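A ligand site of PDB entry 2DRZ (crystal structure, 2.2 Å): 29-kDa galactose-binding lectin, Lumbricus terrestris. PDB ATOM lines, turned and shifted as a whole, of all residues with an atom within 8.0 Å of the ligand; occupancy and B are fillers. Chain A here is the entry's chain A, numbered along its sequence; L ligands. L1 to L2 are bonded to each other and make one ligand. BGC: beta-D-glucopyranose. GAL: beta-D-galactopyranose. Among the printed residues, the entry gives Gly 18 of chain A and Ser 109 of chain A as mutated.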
ATOM      1  N   VAL A  14      -0.488  33.931  -4.569  1.00  0.00           N
ATOM      2  CA  VAL A  14      -0.236  33.442  -3.222  1.00  0.00           C
ATOM      3  C   VAL A  14       0.970  32.509  -3.075  1.00  0.00           C
ATOM      4  O   VAL A  14       1.339  31.809  -4.016  1.00  0.00           O
ATOM      5  CB  VAL A  14      -1.470  32.677  -2.704  1.00  0.00           C
ATOM      6  CG1 VAL A  14      -2.708  33.552  -2.798  1.00  0.00           C
ATOM      7  CG2 VAL A  14      -1.656  31.403  -3.516  1.00  0.00           C
ATOM      8  N   LEU A  15       1.567  32.498  -1.887  1.00  0.00           N
ATOM      9  CA  LEU A  15       2.706  31.621  -1.648  1.00  0.00           C
ATOM     10  C   LEU A  15       2.228  30.226  -2.009  1.00  0.00           C
ATOM     11  O   LEU A  15       1.101  29.828  -1.697  1.00  0.00           O
ATOM     12  CB  LEU A  15       3.172  31.706  -0.189  1.00  0.00           C
ATOM     13  CG  LEU A  15       3.540  33.116   0.325  1.00  0.00           C
ATOM     14  CD1 LEU A  15       4.622  32.994   1.365  1.00  0.00           C
ATOM     15  CD2 LEU A  15       4.016  33.996  -0.799  1.00  0.00           C
ATOM     16  N   ASP A  16       3.103  29.478  -2.674  1.00  0.00           N
ATOM     17  CA  ASP A  16       2.757  28.171  -3.181  1.00  0.00           C
ATOM     18  C   ASP A  16       4.021  27.321  -3.280  1.00  0.00           C
ATOM     19  O   ASP A  16       5.037  27.778  -3.806  1.00  0.00           O
ATOM     20  CB  ASP A  16       2.121  28.405  -4.572  1.00  0.00           C
ATOM     21  CG  ASP A  16       1.887  27.128  -5.348  1.00  0.00           C
ATOM     22  OD1 ASP A  16       2.862  26.402  -5.621  1.00  0.00           O
ATOM     23  OD2 ASP A  16       0.708  26.880  -5.705  1.00  0.00           O
ATOM     24  N   ILE A  17       3.962  26.091  -2.776  1.00  0.00           N
ATOM     25  CA  ILE A  17       5.116  25.207  -2.835  1.00  0.00           C
ATOM     26  C   ILE A  17       5.216  24.669  -4.267  1.00  0.00           C
ATOM     27  O   ILE A  17       4.350  23.920  -4.715  1.00  0.00           O
ATOM     28  CB  ILE A  17       4.995  24.031  -1.844  1.00  0.00           C
ATOM     29  CG1 ILE A  17       4.845  24.564  -0.414  1.00  0.00           C
ATOM     30  CG2 ILE A  17       6.253  23.161  -1.911  1.00  0.00           C
ATOM     31  CD1 ILE A  17       4.692  23.486   0.643  1.00  0.00           C
ATOM     32  N   GLY A  18       6.272  25.085  -4.953  1.00  0.00           N
ATOM     33  CA  GLY A  18       6.507  24.704  -6.332  1.00  0.00           C
ATOM     34  C   GLY A  18       6.191  23.303  -6.795  1.00  0.00           C
ATOM     35  O   GLY A  18       6.867  22.333  -6.434  1.00  0.00           O
ATOM     36  N   GLY A  19       5.146  23.196  -7.622  1.00  0.00           N
ATOM     37  CA  GLY A  19       4.743  21.909  -8.152  1.00  0.00           C
ATOM     38  C   GLY A  19       4.250  20.928  -7.116  1.00  0.00           C
ATOM     39  O   GLY A  19       4.361  19.721  -7.289  1.00  0.00           O
ATOM     40  N   GLN A  20       3.696  21.451  -6.024  1.00  0.00           N
ATOM     41  CA  GLN A  20       3.179  20.611  -4.954  1.00  0.00           C
ATOM     42  C   GLN A  20       4.260  19.692  -4.419  1.00  0.00           C
ATOM     43  O   GLN A  20       3.971  18.731  -3.699  1.00  0.00           O
ATOM     44  CB  GLN A  20       2.006  19.773  -5.459  1.00  0.00           C
ATOM     45  CG  GLN A  20       0.756  20.593  -5.756  1.00  0.00           C
ATOM     46  CD  GLN A  20      -0.229  19.862  -6.645  1.00  0.00           C
ATOM     47  OE1 GLN A  20       0.167  18.685  -7.136  1.00  0.00           O
ATOM     48  NE2 GLN A  20      -1.331  20.346  -6.905  1.00  0.00           N
ATOM     49  N   ASN A  21       5.520  19.982  -4.747  1.00  0.00           N
ATOM     50  CA  ASN A  21       6.614  19.158  -4.270  1.00  0.00           C
ATOM     51  C   ASN A  21       6.595  19.117  -2.737  1.00  0.00           C
ATOM     52  O   ASN A  21       6.692  20.152  -2.067  1.00  0.00           O
ATOM     53  CB  ASN A  21       7.958  19.730  -4.741  1.00  0.00           C
ATOM     54  CG  ASN A  21       9.052  18.695  -4.715  1.00  0.00           C
ATOM     55  OD1 ASN A  21       9.172  17.930  -3.767  1.00  0.00           O
ATOM     56  ND2 ASN A  21       9.871  18.678  -5.751  1.00  0.00           N
ATOM     57  N   LYS A  27      11.268  25.012  -3.553  1.00  0.00           N
ATOM     58  CA  LYS A  27      11.128  26.459  -3.631  1.00  0.00           C
ATOM     59  C   LYS A  27       9.689  26.900  -3.461  1.00  0.00           C
ATOM     60  O   LYS A  27       8.753  26.227  -3.911  1.00  0.00           O
ATOM     61  CB  LYS A  27      11.669  26.993  -4.968  1.00  0.00           C
ATOM     62  CG  LYS A  27      10.796  26.680  -6.185  1.00  0.00           C
ATOM     63  CD  LYS A  27      11.503  27.010  -7.507  1.00  0.00           C
ATOM     64  CE  LYS A  27      11.606  28.518  -7.785  1.00  0.00           C
ATOM     65  NZ  LYS A  27      12.415  29.253  -6.774  1.00  0.00           N
ATOM     66  N   ILE A  29       6.991  29.721  -4.345  1.00  0.00           N
ATOM     67  CA  ILE A  29       6.723  30.755  -5.335  1.00  0.00           C
ATOM     68  C   ILE A  29       5.363  31.377  -5.085  1.00  0.00           C
ATOM     69  O   ILE A  29       4.725  31.094  -4.066  1.00  0.00           O
ATOM     70  CB  ILE A  29       6.699  30.160  -6.768  1.00  0.00           C
ATOM     71  CG1 ILE A  29       5.605  29.081  -6.857  1.00  0.00           C
ATOM     72  CG2 ILE A  29       8.046  29.545  -7.112  1.00  0.00           C
ATOM     73  CD1 ILE A  29       5.394  28.543  -8.257  1.00  0.00           C
ATOM     74  N   THR A  30       4.913  32.231  -5.998  1.00  0.00           N
ATOM     75  CA  THR A  30       3.587  32.831  -5.921  1.00  0.00           C
ATOM     76  C   THR A  30       2.889  32.247  -7.126  1.00  0.00           C
ATOM     77  O   THR A  30       3.498  32.113  -8.194  1.00  0.00           O
ATOM     78  CB  THR A  30       3.599  34.362  -6.036  1.00  0.00           C
ATOM     79  OG1 THR A  30       4.097  34.735  -7.326  1.00  0.00           O
ATOM     80  CG2 THR A  30       4.442  34.974  -4.951  1.00  0.00           C
ATOM     81  N   TRP A  31       1.620  31.894  -6.970  1.00  0.00           N
ATOM     82  CA  TRP A  31       0.854  31.267  -8.037  1.00  0.00           C
ATOM     83  C   TRP A  31      -0.623  31.602  -7.892  1.00  0.00           C
ATOM     84  O   TRP A  31      -1.075  32.005  -6.818  1.00  0.00           O
ATOM     85  CB  TRP A  31       1.092  29.742  -7.951  1.00  0.00           C
ATOM     86  CG  TRP A  31       0.421  28.925  -8.997  1.00  0.00           C
ATOM     87  CD1 TRP A  31      -0.833  28.365  -8.942  1.00  0.00           C
ATOM     88  CD2 TRP A  31       0.978  28.523 -10.252  1.00  0.00           C
ATOM     89  NE1 TRP A  31      -1.078  27.643 -10.080  1.00  0.00           N
ATOM     90  CE2 TRP A  31       0.008  27.724 -10.906  1.00  0.00           C
ATOM     91  CE3 TRP A  31       2.205  28.764 -10.892  1.00  0.00           C
ATOM     92  CZ2 TRP A  31       0.228  27.168 -12.170  1.00  0.00           C
ATOM     93  CZ3 TRP A  31       2.424  28.216 -12.150  1.00  0.00           C
ATOM     94  CH2 TRP A  31       1.438  27.419 -12.771  1.00  0.00           C
ATOM     95  N   ASP A  32      -1.387  31.461  -8.969  1.00  0.00           N
ATOM     96  CA  ASP A  32      -2.801  31.761  -8.893  1.00  0.00           C
ATOM     97  C   ASP A  32      -3.458  30.963  -7.778  1.00  0.00           C
ATOM     98  O   ASP A  32      -3.280  29.755  -7.664  1.00  0.00           O
ATOM     99  CB  ASP A  32      -3.500  31.483 -10.220  1.00  0.00           C
ATOM    100  CG  ASP A  32      -3.133  32.485 -11.292  1.00  0.00           C
ATOM    101  OD1 ASP A  32      -3.050  33.687 -10.963  1.00  0.00           O
ATOM    102  OD2 ASP A  32      -2.930  32.086 -12.450  1.00  0.00           O
ATOM    103  N   GLN A  33      -4.213  31.670  -6.947  1.00  0.00           N
ATOM    104  CA  GLN A  33      -4.908  31.073  -5.823  1.00  0.00           C
ATOM    105  C   GLN A  33      -5.875  29.982  -6.263  1.00  0.00           C
ATOM    106  O   GLN A  33      -6.887  30.259  -6.906  1.00  0.00           O
ATOM    107  CB  GLN A  33      -5.663  32.162  -5.066  1.00  0.00           C
ATOM    108  CG  GLN A  33      -6.574  31.667  -3.971  1.00  0.00           C
ATOM    109  CD  GLN A  33      -7.034  32.809  -3.098  1.00  0.00           C
ATOM    110  OE1 GLN A  33      -7.357  33.887  -3.584  1.00  0.00           O
ATOM    111  NE2 GLN A  33      -7.066  32.579  -1.780  1.00  0.00           N
ATOM    112  N   LYS A  34      -5.549  28.740  -5.913  1.00  0.00           N
ATOM    113  CA  LYS A  34      -6.385  27.595  -6.241  1.00  0.00           C
ATOM    114  C   LYS A  34      -7.388  27.368  -5.118  1.00  0.00           C
ATOM    115  O   LYS A  34      -7.222  27.891  -4.011  1.00  0.00           O
ATOM    116  CB  LYS A  34      -5.526  26.338  -6.388  1.00  0.00           C
ATOM    117  CG  LYS A  34      -4.569  26.346  -7.560  1.00  0.00           C
ATOM    118  CD  LYS A  34      -3.761  25.058  -7.605  1.00  0.00           C
ATOM    119  CE  LYS A  34      -2.859  24.922  -6.373  1.00  0.00           C
ATOM    120  NZ  LYS A  34      -2.093  23.647  -6.408  1.00  0.00           N
ATOM    121  N   THR A  38      -6.923  20.690  -3.824  1.00  0.00           N
ATOM    122  CA  THR A  38      -5.710  20.875  -4.608  1.00  0.00           C
ATOM    123  C   THR A  38      -4.923  22.097  -4.123  1.00  0.00           C
ATOM    124  O   THR A  38      -3.780  22.315  -4.543  1.00  0.00           O
ATOM    125  CB  THR A  38      -6.032  21.071  -6.102  1.00  0.00           C
ATOM    126  OG1 THR A  38      -6.748  22.300  -6.277  1.00  0.00           O
ATOM    127  CG2 THR A  38      -6.894  19.928  -6.613  1.00  0.00           C
ATOM    128  N   ALA A  39      -5.542  22.885  -3.251  1.00  0.00           N
ATOM    129  CA  ALA A  39      -4.927  24.100  -2.722  1.00  0.00           C
ATOM    130  C   ALA A  39      -3.974  23.842  -1.555  1.00  0.00           C
ATOM    131  O   ALA A  39      -3.337  24.764  -1.060  1.00  0.00           O
ATOM    132  CB  ALA A  39      -6.008  25.074  -2.294  1.00  0.00           C
ATOM    133  N   VAL A  40      -3.874  22.587  -1.140  1.00  0.00           N
ATOM    134  CA  VAL A  40      -3.027  22.240  -0.013  1.00  0.00           C
ATOM    135  C   VAL A  40      -1.622  22.866  -0.057  1.00  0.00           C
ATOM    136  O   VAL A  40      -1.144  23.376   0.963  1.00  0.00           O
ATOM    137  CB  VAL A  40      -2.911  20.707   0.126  1.00  0.00           C
ATOM    138  CG1 VAL A  40      -2.229  20.128  -1.106  1.00  0.00           C
ATOM    139  CG2 VAL A  40      -2.142  20.361   1.393  1.00  0.00           C
ATOM    140  N   ASN A  41      -0.971  22.865  -1.225  1.00  0.00           N
ATOM    141  CA  ASN A  41       0.371  23.441  -1.312  1.00  0.00           C
ATOM    142  C   ASN A  41       0.351  24.962  -1.261  1.00  0.00           C
ATOM    143  O   ASN A  41       1.388  25.611  -1.401  1.00  0.00           O
ATOM    144  CB  ASN A  41       1.094  22.951  -2.588  1.00  0.00           C
ATOM    145  CG  ASN A  41       0.524  23.552  -3.860  1.00  0.00           C
ATOM    146  OD1 ASN A  41      -0.686  23.526  -4.086  1.00  0.00           O
ATOM    147  ND2 ASN A  41       1.401  24.076  -4.717  1.00  0.00           N
ATOM    148  N   GLN A  42      -0.830  25.528  -1.044  1.00  0.00           N
ATOM    149  CA  GLN A  42      -0.983  26.975  -0.947  1.00  0.00           C
ATOM    150  C   GLN A  42      -1.580  27.359   0.409  1.00  0.00           C
ATOM    151  O   GLN A  42      -1.861  28.533   0.670  1.00  0.00           O
ATOM    152  CB  GLN A  42      -1.902  27.500  -2.049  1.00  0.00           C
ATOM    153  CG  GLN A  42      -1.510  27.112  -3.449  1.00  0.00           C
ATOM    154  CD  GLN A  42      -2.358  27.824  -4.482  1.00  0.00           C
ATOM    155  OE1 GLN A  42      -3.545  28.062  -4.266  1.00  0.00           O
ATOM    156  NE2 GLN A  42      -1.758  28.148  -5.615  1.00  0.00           N
ATOM    157  N   SER A 109       7.384  31.687 -12.698  1.00  0.00           N
ATOM    158  CA  SER A 109       6.645  32.192 -11.547  1.00  0.00           C
ATOM    159  C   SER A 109       7.610  32.967 -10.658  1.00  0.00           C
ATOM    160  O   SER A 109       8.802  32.651 -10.587  1.00  0.00           O
ATOM    161  CB  SER A 109       6.041  31.038 -10.748  1.00  0.00           C
ATOM    162  OG  SER A 109       5.160  30.264 -11.548  1.00  0.00           O
HETATM  163  C2  BGC L   1       3.456  20.551 -13.340  1.00  0.00           C
HETATM  164  C3  BGC L   1       3.303  21.248 -11.988  1.00  0.00           C
HETATM  165  C4  BGC L   1       1.886  20.938 -11.477  1.00  0.00           C
HETATM  166  C5  BGC L   1       1.723  19.409 -11.369  1.00  0.00           C
HETATM  167  C6  BGC L   1       0.349  18.988 -10.882  1.00  0.00           C
HETATM  168  C1  BGC L   1       3.243  19.045 -13.180  1.00  0.00           C
HETATM  169  O1  BGC L   1       3.317  18.443 -14.430  1.00  0.00           O
HETATM  170  O2  BGC L   1       4.762  20.808 -13.858  1.00  0.00           O
HETATM  171  O3  BGC L   1       3.460  22.641 -12.182  1.00  0.00           O
HETATM  172  O4  BGC L   1       1.564  21.562 -10.205  1.00  0.00           O
HETATM  173  O5  BGC L   1       1.936  18.796 -12.657  1.00  0.00           O
HETATM  174  O6  BGC L   1      -0.629  19.966 -11.205  1.00  0.00           O
HETATM  175  C1  GAL L   2       1.411  22.941 -10.112  1.00  0.00           C
HETATM  176  C2  GAL L   2       0.887  23.300  -8.722  1.00  0.00           C
HETATM  177  C3  GAL L   2       0.749  24.815  -8.639  1.00  0.00           C
HETATM  178  C4  GAL L   2       2.105  25.450  -8.901  1.00  0.00           C
HETATM  179  C5  GAL L   2       2.604  25.023 -10.279  1.00  0.00           C
HETATM  180  C6  GAL L   2       4.000  25.560 -10.547  1.00  0.00           C
HETATM  181  O2  GAL L   2      -0.377  22.691  -8.508  1.00  0.00           O
HETATM  182  O3  GAL L   2       0.278  25.187  -7.360  1.00  0.00           O
HETATM  183  O4  GAL L   2       3.037  25.037  -7.906  1.00  0.00           O
HETATM  184  O5  GAL L   2       2.680  23.574 -10.346  1.00  0.00           O
HETATM  185  O6  GAL L   2       4.448  25.262 -11.855  1.00  0.00           O
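The side-chain carboxylate (OD2) of Asp 16 is in hydrogen-bond range of an oxygen (O3) of GAL L2 (2.4 Å).
N of Gly 19 lies within hydrogen-bond range of O4 of GAL L2 (2.8 Å).
NZ of Lys 34 sits at hydrogen-bond distance from O2 of GAL L2 (2.9 Å).
The side-chain amide nitrogen (NE2) of Gln 20 lies within hydrogen-bond range of an oxygen (O2) of GAL L2, 3.0 Å away.
The side-chain amide nitrogen (ND2) of Asn 41 is in hydrogen-bond range of an oxygen (O3) of GAL L2 (3.1 Å).
The side-chain carboxylate (OD1) of Asp 16 is in hydrogen-bond range of the side-chain amide nitrogen (ND2) of Asn 41, at 2.9 Å.
OD2 of Asp 16 sits at hydrogen-bond distance from NE2 of Gln 42.
The backbone carbonyl oxygen (O) of Ile 29 is in hydrogen-bond range of the backbone NH (N) of Asp 16.
The backbone NH of Lys 34 lies within hydrogen-bond range of the side-chain amide oxygen of Gln 42 (2.7 Å).
ND2 of Asn 41 lies within hydrogen-bond range of O of Ile 17, at 3.0 Å.
OD1 of Asn 41 sits close to O of Thr 38.
The backbone carbonyl oxygen (O) of Lys 27 is in hydrogen-bond range of the backbone NH (N) of Gly 18 (2.9 Å).
The side-chain amide nitrogen (NE2) of Gln 42 lies within hydrogen-bond range of the backbone carbonyl oxygen (O) of Asp 32.
O of Ile 17 touches O4 of GAL L2 (3.6 Å).
C of Gly 18 touches O4 of GAL L2, 3.8 Å away.
CZ3 of Trp 31 touches C6 of GAL L2, 3.5 Å away.
NE2 of Gln 42 touches O3 of GAL L2 (3.99 Å).
Hydrophobic or aromatic side chains within 4 Å of the ligand: Trp 31.
Nine residues have an atom within 4 Å of the ligand: Asp 16, Ile 17, Gly 18, Gly 19, Gln 20, Trp 31, Lys 34, Asn 41 and Gln 42.
The nearest printed residue that does not touch the ligand is Ile 29 (4.01 Å).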
